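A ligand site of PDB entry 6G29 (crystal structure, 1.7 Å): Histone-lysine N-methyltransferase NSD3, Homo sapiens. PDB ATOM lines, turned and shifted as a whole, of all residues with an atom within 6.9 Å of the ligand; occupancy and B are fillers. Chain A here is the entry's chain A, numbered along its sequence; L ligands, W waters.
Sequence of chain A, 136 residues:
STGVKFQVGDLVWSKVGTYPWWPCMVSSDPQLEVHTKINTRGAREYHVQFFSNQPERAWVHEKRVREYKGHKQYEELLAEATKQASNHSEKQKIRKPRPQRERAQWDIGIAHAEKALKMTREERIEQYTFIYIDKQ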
ATOM      1  N   SER A  14     -21.052 -20.829 -10.276  1.00  0.00           N
ATOM      2  CA  SER A  14     -22.362 -21.246 -10.818  1.00  0.00           C
ATOM      3  C   SER A  14     -22.826 -20.174 -11.791  1.00  0.00           C
ATOM      4  O   SER A  14     -22.730 -19.002 -11.460  1.00  0.00           O
ATOM      5  CB  SER A  14     -23.404 -21.371  -9.711  1.00  0.00           C
ATOM      6  OG  SER A  14     -22.982 -22.283  -8.716  1.00  0.00           O
ATOM      7  N   LYS A  15     -23.402 -20.593 -12.938  1.00  0.00           N
ATOM      8  CA  LYS A  15     -23.930 -19.662 -13.945  1.00  0.00           C
ATOM      9  C   LYS A  15     -25.435 -19.878 -13.947  1.00  0.00           C
ATOM     10  O   LYS A  15     -25.900 -20.934 -14.379  1.00  0.00           O
ATOM     11  CB  LYS A  15     -23.295 -19.956 -15.321  1.00  0.00           C
ATOM     12  CG  LYS A  15     -23.737 -19.032 -16.445  1.00  0.00           C
ATOM     13  CD  LYS A  15     -23.069 -17.672 -16.420  1.00  0.00           C
ATOM     14  CE  LYS A  15     -23.515 -16.840 -17.614  1.00  0.00           C
ATOM     15  NZ  LYS A  15     -24.910 -16.328 -17.444  1.00  0.00           N
ATOM     16  N   VAL A  16     -26.179 -18.924 -13.393  1.00  0.00           N
ATOM     17  CA  VAL A  16     -27.639 -19.051 -13.250  1.00  0.00           C
ATOM     18  C   VAL A  16     -28.362 -17.894 -13.912  1.00  0.00           C
ATOM     19  O   VAL A  16     -28.057 -16.741 -13.629  1.00  0.00           O
ATOM     20  CB  VAL A  16     -28.066 -19.168 -11.748  1.00  0.00           C
ATOM     21  CG1 VAL A  16     -29.540 -19.536 -11.616  1.00  0.00           C
ATOM     22  CG2 VAL A  16     -27.195 -20.159 -10.967  1.00  0.00           C
ATOM     23  N   GLY A  17     -29.366 -18.224 -14.745  1.00  0.00           N
ATOM     24  CA  GLY A  17     -30.219 -17.264 -15.423  1.00  0.00           C
ATOM     25  C   GLY A  17     -29.498 -16.083 -16.048  1.00  0.00           C
ATOM     26  O   GLY A  17     -28.623 -16.276 -16.878  1.00  0.00           O
ATOM     27  N   THR A  18     -29.828 -14.861 -15.590  1.00  0.00           N
ATOM     28  CA  THR A  18     -29.238 -13.638 -16.148  1.00  0.00           C
ATOM     29  C   THR A  18     -27.932 -13.220 -15.461  1.00  0.00           C
ATOM     30  O   THR A  18     -27.316 -12.232 -15.847  1.00  0.00           O
ATOM     31  CB  THR A  18     -30.245 -12.477 -16.091  1.00  0.00           C
ATOM     32  OG1 THR A  18     -30.528 -12.155 -14.728  1.00  0.00           O
ATOM     33  CG2 THR A  18     -31.530 -12.772 -16.844  1.00  0.00           C
ATOM     34  N   TYR A  19     -27.507 -13.953 -14.422  1.00  0.00           N
ATOM     35  CA  TYR A  19     -26.332 -13.591 -13.638  1.00  0.00           C
ATOM     36  C   TYR A  19     -25.028 -14.079 -14.258  1.00  0.00           C
ATOM     37  O   TYR A  19     -25.029 -15.128 -14.902  1.00  0.00           O
ATOM     38  CB  TYR A  19     -26.474 -14.147 -12.216  1.00  0.00           C
ATOM     39  CG  TYR A  19     -27.619 -13.510 -11.456  1.00  0.00           C
ATOM     40  CD1 TYR A  19     -27.421 -12.335 -10.743  1.00  0.00           C
ATOM     41  CD2 TYR A  19     -28.892 -14.068 -11.483  1.00  0.00           C
ATOM     42  CE1 TYR A  19     -28.475 -11.731 -10.049  1.00  0.00           C
ATOM     43  CE2 TYR A  19     -29.948 -13.488 -10.770  1.00  0.00           C
ATOM     44  CZ  TYR A  19     -29.729 -12.310 -10.066  1.00  0.00           C
ATOM     45  OH  TYR A  19     -30.767 -11.721  -9.374  1.00  0.00           O
ATOM     46  N   PRO A  20     -23.894 -13.387 -14.011  1.00  0.00           N
ATOM     47  CA  PRO A  20     -22.607 -13.885 -14.522  1.00  0.00           C
ATOM     48  C   PRO A  20     -22.129 -15.076 -13.684  1.00  0.00           C
ATOM     49  O   PRO A  20     -22.689 -15.333 -12.600  1.00  0.00           O
ATOM     50  CB  PRO A  20     -21.672 -12.696 -14.310  1.00  0.00           C
ATOM     51  CG  PRO A  20     -22.210 -12.041 -13.077  1.00  0.00           C
ATOM     52  CD  PRO A  20     -23.708 -12.140 -13.227  1.00  0.00           C
ATOM     53  N   TRP A  21     -21.076 -15.785 -14.136  1.00  0.00           N
ATOM     54  CA  TRP A  21     -20.486 -16.869 -13.326  1.00  0.00           C
ATOM     55  C   TRP A  21     -20.240 -16.297 -11.930  1.00  0.00           C
ATOM     56  O   TRP A  21     -19.670 -15.203 -11.801  1.00  0.00           O
ATOM     57  CB  TRP A  21     -19.180 -17.330 -13.932  1.00  0.00           C
ATOM     58  CG  TRP A  21     -19.376 -18.164 -15.157  1.00  0.00           C
ATOM     59  CD1 TRP A  21     -19.277 -17.748 -16.455  1.00  0.00           C
ATOM     60  CD2 TRP A  21     -19.680 -19.561 -15.191  1.00  0.00           C
ATOM     61  NE1 TRP A  21     -19.530 -18.809 -17.304  1.00  0.00           N
ATOM     62  CE2 TRP A  21     -19.771 -19.937 -16.558  1.00  0.00           C
ATOM     63  CE3 TRP A  21     -19.876 -20.543 -14.207  1.00  0.00           C
ATOM     64  CZ2 TRP A  21     -20.041 -21.261 -16.958  1.00  0.00           C
ATOM     65  CZ3 TRP A  21     -20.148 -21.843 -14.602  1.00  0.00           C
ATOM     66  CH2 TRP A  21     -20.208 -22.192 -15.966  1.00  0.00           C
ATOM     67  N   TRP A  22     -20.752 -16.977 -10.901  1.00  0.00           N
ATOM     68  CA  TRP A  22     -20.741 -16.469  -9.545  1.00  0.00           C
ATOM     69  C   TRP A  22     -20.051 -17.393  -8.544  1.00  0.00           C
ATOM     70  O   TRP A  22     -20.329 -18.582  -8.561  1.00  0.00           O
ATOM     71  CB  TRP A  22     -22.198 -16.220  -9.097  1.00  0.00           C
ATOM     72  CG  TRP A  22     -22.313 -15.143  -8.066  1.00  0.00           C
ATOM     73  CD1 TRP A  22     -22.130 -15.252  -6.719  1.00  0.00           C
ATOM     74  CD2 TRP A  22     -22.623 -13.769  -8.324  1.00  0.00           C
ATOM     75  NE1 TRP A  22     -22.224 -14.008  -6.131  1.00  0.00           N
ATOM     76  CE2 TRP A  22     -22.566 -13.084  -7.081  1.00  0.00           C
ATOM     77  CE3 TRP A  22     -22.966 -13.046  -9.489  1.00  0.00           C
ATOM     78  CZ2 TRP A  22     -22.823 -11.714  -6.971  1.00  0.00           C
ATOM     79  CZ3 TRP A  22     -23.225 -11.685  -9.375  1.00  0.00           C
ATOM     80  CH2 TRP A  22     -23.159 -11.036  -8.136  1.00  0.00           C
ATOM     81  N   CYS A  24     -19.537 -19.575  -5.345  1.00  0.00           N
ATOM     82  CA  CYS A  24     -20.459 -20.301  -4.464  1.00  0.00           C
ATOM     83  C   CYS A  24     -19.746 -21.285  -3.552  1.00  0.00           C
ATOM     84  O   CYS A  24     -18.621 -21.704  -3.830  1.00  0.00           O
ATOM     85  CB  CYS A  24     -21.480 -21.072  -5.291  1.00  0.00           C
ATOM     86  SG  CYS A  24     -22.454 -20.049  -6.419  1.00  0.00           S
ATOM     87  N   PHE A  50     -24.668 -18.617  -2.676  1.00  0.00           N
ATOM     88  CA  PHE A  50     -23.895 -17.622  -3.418  1.00  0.00           C
ATOM     89  C   PHE A  50     -23.152 -16.741  -2.426  1.00  0.00           C
ATOM     90  O   PHE A  50     -23.788 -16.196  -1.511  1.00  0.00           O
ATOM     91  CB  PHE A  50     -24.828 -16.697  -4.234  1.00  0.00           C
ATOM     92  CG  PHE A  50     -25.617 -17.444  -5.272  1.00  0.00           C
ATOM     93  CD1 PHE A  50     -25.038 -17.766  -6.498  1.00  0.00           C
ATOM     94  CD2 PHE A  50     -26.929 -17.829  -5.039  1.00  0.00           C
ATOM     95  CE1 PHE A  50     -25.753 -18.479  -7.462  1.00  0.00           C
ATOM     96  CE2 PHE A  50     -27.639 -18.564  -5.999  1.00  0.00           C
ATOM     97  CZ  PHE A  50     -27.052 -18.887  -7.194  1.00  0.00           C
ATOM     98  N   PHE A  51     -21.828 -16.574  -2.598  1.00  0.00           N
ATOM     99  CA  PHE A  51     -21.077 -15.621  -1.785  1.00  0.00           C
ATOM    100  C   PHE A  51     -21.490 -14.224  -2.212  1.00  0.00           C
ATOM    101  O   PHE A  51     -21.473 -13.907  -3.417  1.00  0.00           O
ATOM    102  CB  PHE A  51     -19.564 -15.794  -1.945  1.00  0.00           C
ATOM    103  CG  PHE A  51     -18.989 -17.026  -1.306  1.00  0.00           C
ATOM    104  CD1 PHE A  51     -18.817 -17.097   0.078  1.00  0.00           C
ATOM    105  CD2 PHE A  51     -18.552 -18.093  -2.070  1.00  0.00           C
ATOM    106  CE1 PHE A  51     -18.243 -18.225   0.675  1.00  0.00           C
ATOM    107  CE2 PHE A  51     -17.954 -19.214  -1.472  1.00  0.00           C
ATOM    108  CZ  PHE A  51     -17.800 -19.264  -0.099  1.00  0.00           C
ATOM    109  N   SER A  52     -21.831 -13.372  -1.241  1.00  0.00           N
ATOM    110  CA  SER A  52     -22.352 -12.028  -1.524  1.00  0.00           C
ATOM    111  C   SER A  52     -22.609 -11.296  -0.217  1.00  0.00           C
ATOM    112  O   SER A  52     -22.609 -11.921   0.843  1.00  0.00           O
ATOM    113  CB  SER A  52     -23.704 -12.186  -2.240  1.00  0.00           C
ATOM    114  OG  SER A  52     -24.381 -10.970  -2.517  1.00  0.00           O
ATOM    115  N   ASN A  53     -22.950 -10.001  -0.296  1.00  0.00           N
ATOM    116  CA  ASN A  53     -23.365  -9.250   0.886  1.00  0.00           C
ATOM    117  C   ASN A  53     -24.849  -9.578   1.175  1.00  0.00           C
ATOM    118  O   ASN A  53     -25.374  -9.164   2.211  1.00  0.00           O
ATOM    119  CB  ASN A  53     -23.208  -7.741   0.641  1.00  0.00           C
ATOM    120  CG  ASN A  53     -24.087  -7.216  -0.482  1.00  0.00           C
ATOM    121  OD1 ASN A  53     -24.237  -7.841  -1.533  1.00  0.00           O
ATOM    122  ND2 ASN A  53     -24.700  -6.061  -0.278  1.00  0.00           N
ATOM    123  N   GLN A  54     -25.522 -10.295   0.252  1.00  0.00           N
ATOM    124  CA  GLN A  54     -26.940 -10.656   0.262  1.00  0.00           C
ATOM    125  C   GLN A  54     -27.033 -12.211   0.188  1.00  0.00           C
ATOM    126  O   GLN A  54     -26.961 -12.773  -0.916  1.00  0.00           O
ATOM    127  CB  GLN A  54     -27.629  -9.946  -0.930  1.00  0.00           C
ATOM    128  CG  GLN A  54     -29.055 -10.360  -1.299  1.00  0.00           C
ATOM    129  CD  GLN A  54     -29.331 -10.187  -2.787  1.00  0.00           C
ATOM    130  OE1 GLN A  54     -28.867  -9.248  -3.445  1.00  0.00           O
ATOM    131  NE2 GLN A  54     -30.091 -11.094  -3.367  1.00  0.00           N
ATOM    132  N   PRO A  55     -27.165 -12.924   1.345  1.00  0.00           N
ATOM    133  CA  PRO A  55     -27.203 -14.401   1.306  1.00  0.00           C
ATOM    134  C   PRO A  55     -28.351 -14.958   0.483  1.00  0.00           C
ATOM    135  O   PRO A  55     -29.501 -14.563   0.655  1.00  0.00           O
ATOM    136  CB  PRO A  55     -27.315 -14.802   2.780  1.00  0.00           C
ATOM    137  CG  PRO A  55     -27.813 -13.595   3.479  1.00  0.00           C
ATOM    138  CD  PRO A  55     -27.236 -12.429   2.734  1.00  0.00           C
ATOM    139  N   GLU A  56     -28.024 -15.841  -0.462  1.00  0.00           N
ATOM    140  CA  GLU A  56     -29.016 -16.474  -1.341  1.00  0.00           C
ATOM    141  C   GLU A  56     -28.517 -17.857  -1.667  1.00  0.00           C
ATOM    142  O   GLU A  56     -27.324 -18.129  -1.572  1.00  0.00           O
ATOM    143  CB  GLU A  56     -29.193 -15.705  -2.668  1.00  0.00           C
ATOM    144  CG  GLU A  56     -29.859 -14.334  -2.554  1.00  0.00           C
ATOM    145  CD  GLU A  56     -31.372 -14.252  -2.609  1.00  0.00           C
ATOM    146  OE1 GLU A  56     -31.885 -13.147  -2.912  1.00  0.00           O
ATOM    147  OE2 GLU A  56     -32.047 -15.261  -2.340  1.00  0.00           O
ATOM    148  N   ARG A  57     -29.443 -18.717  -2.070  1.00  0.00           N
ATOM    149  CA  ARG A  57     -29.098 -20.094  -2.409  1.00  0.00           C
ATOM    150  C   ARG A  57     -29.894 -20.519  -3.608  1.00  0.00           C
ATOM    151  O   ARG A  57     -30.904 -19.873  -3.936  1.00  0.00           O
ATOM    152  CB  ARG A  57     -29.395 -21.021  -1.218  1.00  0.00           C
ATOM    153  CG  ARG A  57     -30.873 -20.950  -0.763  1.00  0.00           C
ATOM    154  CD  ARG A  57     -31.202 -21.983   0.272  1.00  0.00           C
ATOM    155  NE  ARG A  57     -32.645 -22.147   0.442  1.00  0.00           N
ATOM    156  CZ  ARG A  57     -33.341 -23.150  -0.067  1.00  0.00           C
ATOM    157  NH1 ARG A  57     -34.653 -23.240   0.144  1.00  0.00           N
ATOM    158  NH2 ARG A  57     -32.745 -24.085  -0.795  1.00  0.00           N
ATOM    159  N   ALA A  58     -29.499 -21.633  -4.231  1.00  0.00           N
ATOM    160  CA  ALA A  58     -30.240 -22.161  -5.386  1.00  0.00           C
ATOM    161  C   ALA A  58     -29.804 -23.565  -5.716  1.00  0.00           C
ATOM    162  O   ALA A  58     -28.695 -23.976  -5.372  1.00  0.00           O
ATOM    163  CB  ALA A  58     -30.005 -21.300  -6.612  1.00  0.00           C
ATOM    164  N   GLU A 102     -24.337  -4.949  -9.587  1.00  0.00           N
ATOM    165  CA  GLU A 102     -24.050  -6.375  -9.682  1.00  0.00           C
ATOM    166  C   GLU A 102     -22.544  -6.635  -9.525  1.00  0.00           C
ATOM    167  O   GLU A 102     -22.173  -7.533  -8.781  1.00  0.00           O
ATOM    168  CB  GLU A 102     -24.568  -6.925 -11.030  1.00  0.00           C
ATOM    169  CG  GLU A 102     -24.591  -8.444 -11.084  1.00  0.00           C
ATOM    170  CD  GLU A 102     -25.120  -8.941 -12.412  1.00  0.00           C
ATOM    171  OE1 GLU A 102     -24.393  -8.834 -13.423  1.00  0.00           O
ATOM    172  OE2 GLU A 102     -26.283  -9.417 -12.448  1.00  0.00           O
ATOM    173  N   GLN A 105     -21.446  -6.336  -5.858  1.00  0.00           N
ATOM    174  CA  GLN A 105     -21.912  -7.503  -5.141  1.00  0.00           C
ATOM    175  C   GLN A 105     -20.984  -8.669  -5.488  1.00  0.00           C
ATOM    176  O   GLN A 105     -20.591  -9.425  -4.584  1.00  0.00           O
ATOM    177  CB  GLN A 105     -23.350  -7.808  -5.604  1.00  0.00           C
ATOM    178  CG  GLN A 105     -24.177  -8.603  -4.649  1.00  0.00           C
ATOM    179  CD  GLN A 105     -25.642  -8.246  -4.727  1.00  0.00           C
ATOM    180  OE1 GLN A 105     -26.217  -8.088  -5.816  1.00  0.00           O
ATOM    181  NE2 GLN A 105     -26.277  -8.137  -3.582  1.00  0.00           N
ATOM    182  N   TRP A 106     -20.607  -8.806  -6.796  1.00  0.00           N
ATOM    183  CA  TRP A 106     -19.714  -9.871  -7.271  1.00  0.00           C
ATOM    184  C   TRP A 106     -18.320  -9.720  -6.636  1.00  0.00           C
ATOM    185  O   TRP A 106     -17.753 -10.696  -6.159  1.00  0.00           O
ATOM    186  CB  TRP A 106     -19.640  -9.854  -8.805  1.00  0.00           C
ATOM    187  CG  TRP A 106     -18.887 -11.000  -9.426  1.00  0.00           C
ATOM    188  CD1 TRP A 106     -19.404 -12.194  -9.853  1.00  0.00           C
ATOM    189  CD2 TRP A 106     -17.504 -11.004  -9.789  1.00  0.00           C
ATOM    190  NE1 TRP A 106     -18.427 -12.938 -10.466  1.00  0.00           N
ATOM    191  CE2 TRP A 106     -17.251 -12.232 -10.449  1.00  0.00           C
ATOM    192  CE3 TRP A 106     -16.461 -10.057  -9.697  1.00  0.00           C
ATOM    193  CZ2 TRP A 106     -15.984 -12.558 -10.949  1.00  0.00           C
ATOM    194  CZ3 TRP A 106     -15.203 -10.396 -10.179  1.00  0.00           C
ATOM    195  CH2 TRP A 106     -14.971 -11.632 -10.785  1.00  0.00           C
HETATM  196  C1  LIG L   1     -29.463 -16.331  -8.820  1.00  0.00           C
HETATM  197  C2  LIG L   1     -27.937 -14.597  -7.261  1.00  0.00           C
HETATM  198  C3  LIG L   1     -26.695 -12.470  -6.789  1.00  0.00           C
HETATM  199  N1  LIG L   1     -26.005 -11.900  -4.569  1.00  0.00           N
HETATM  200  C4  LIG L   1     -26.561 -13.040  -4.148  1.00  0.00           C
HETATM  201  C5  LIG L   1     -31.338 -15.835  -7.225  1.00  0.00           C
HETATM  202  C6  LIG L   1     -33.420 -14.688  -6.480  1.00  0.00           C
HETATM  203  C7  LIG L   1     -31.330 -16.633  -5.928  1.00  0.00           C
HETATM  204  C8  LIG L   1     -25.857 -15.062  -8.773  1.00  0.00           C
HETATM  205  C9  LIG L   1     -27.310 -15.242  -8.418  1.00  0.00           C
HETATM  206  C10 LIG L   1     -28.087 -16.087  -9.133  1.00  0.00           C
HETATM  207  O1  LIG L   1     -30.207 -17.052  -9.473  1.00  0.00           O
HETATM  208  N2  LIG L   1     -29.954 -15.650  -7.722  1.00  0.00           N
HETATM  209  N3  LIG L   1     -29.183 -14.804  -6.950  1.00  0.00           N
HETATM  210  C11 LIG L   1     -27.214 -13.677  -6.350  1.00  0.00           C
HETATM  211  C12 LIG L   1     -26.121 -11.615  -5.872  1.00  0.00           C
HETATM  212  C13 LIG L   1     -27.156 -13.959  -4.984  1.00  0.00           C
HETATM  213  C14 LIG L   1     -32.026 -14.487  -7.041  1.00  0.00           C
HETATM  214  N4  LIG L   1     -33.374 -15.450  -5.208  1.00  0.00           N
HETATM  215  C15 LIG L   1     -32.736 -16.786  -5.388  1.00  0.00           C
HETATM  216  O   HOH W   1     -33.343 -13.064  -9.933  1.00  0.00           O
HETATM  217  O   HOH W   2     -32.018 -16.543 -11.483  1.00  0.00           O
HETATM  218  O   HOH W   3     -31.939 -19.123  -8.803  1.00  0.00           O
HETATM  219  O   HOH W   4     -33.026 -20.082  -5.828  1.00  0.00           O
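The side-chain hydroxyl of Ser 52 is in hydrogen-bond range of a nitrogen (N1) of the ligand (2.8 Å). The side-chain carboxylate of Glu 56 is in salt-bridge range of a nitrogen (N4) of the ligand (3.2 Å).
O of Trp 22 lies within hydrogen-bond range of SG of Cys 24 (3.4 Å). The side-chain amide nitrogen of Gln 105 is in hydrogen-bond range of the side-chain amide oxygen of Gln 54 (2.8 Å). N of Trp 22 sits at hydrogen-bond distance from O of Ser 14 (2.9 Å). NE2 of Gln 54 lies within hydrogen-bond range of OE1 of Glu 56 (2.8 Å). NE1 of Trp 22 sits at hydrogen-bond distance from O of Phe 51. The backbone carbonyl oxygen of Tyr 19 sits at hydrogen-bond distance from the side-chain amino group of Lys 15 (2.8 Å). N of Phe 50 sits at hydrogen-bond distance from O of Glu 56, at 2.9 Å. OG of Ser 52 is in hydrogen-bond range of N of Gln 54 (3.1 Å).
Val 16 touches the ligand (CG1 to O1, 3.3 Å). Tyr 19 touches the ligand. Trp 22 touches the ligand. Phe 50 touches the ligand (CZ to C10, 3.6 Å). O of Gln 54 touches C4 of the ligand, 3.3 Å away. Arg 57 touches the ligand (O to C7, 3.8 Å). OE1 of Gln 105 touches C12 of the ligand (3.5 Å). Hydrophobic or aromatic side chains within 4 Å of the ligand: Val 16, Tyr 19, Trp 22 and Phe 50.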
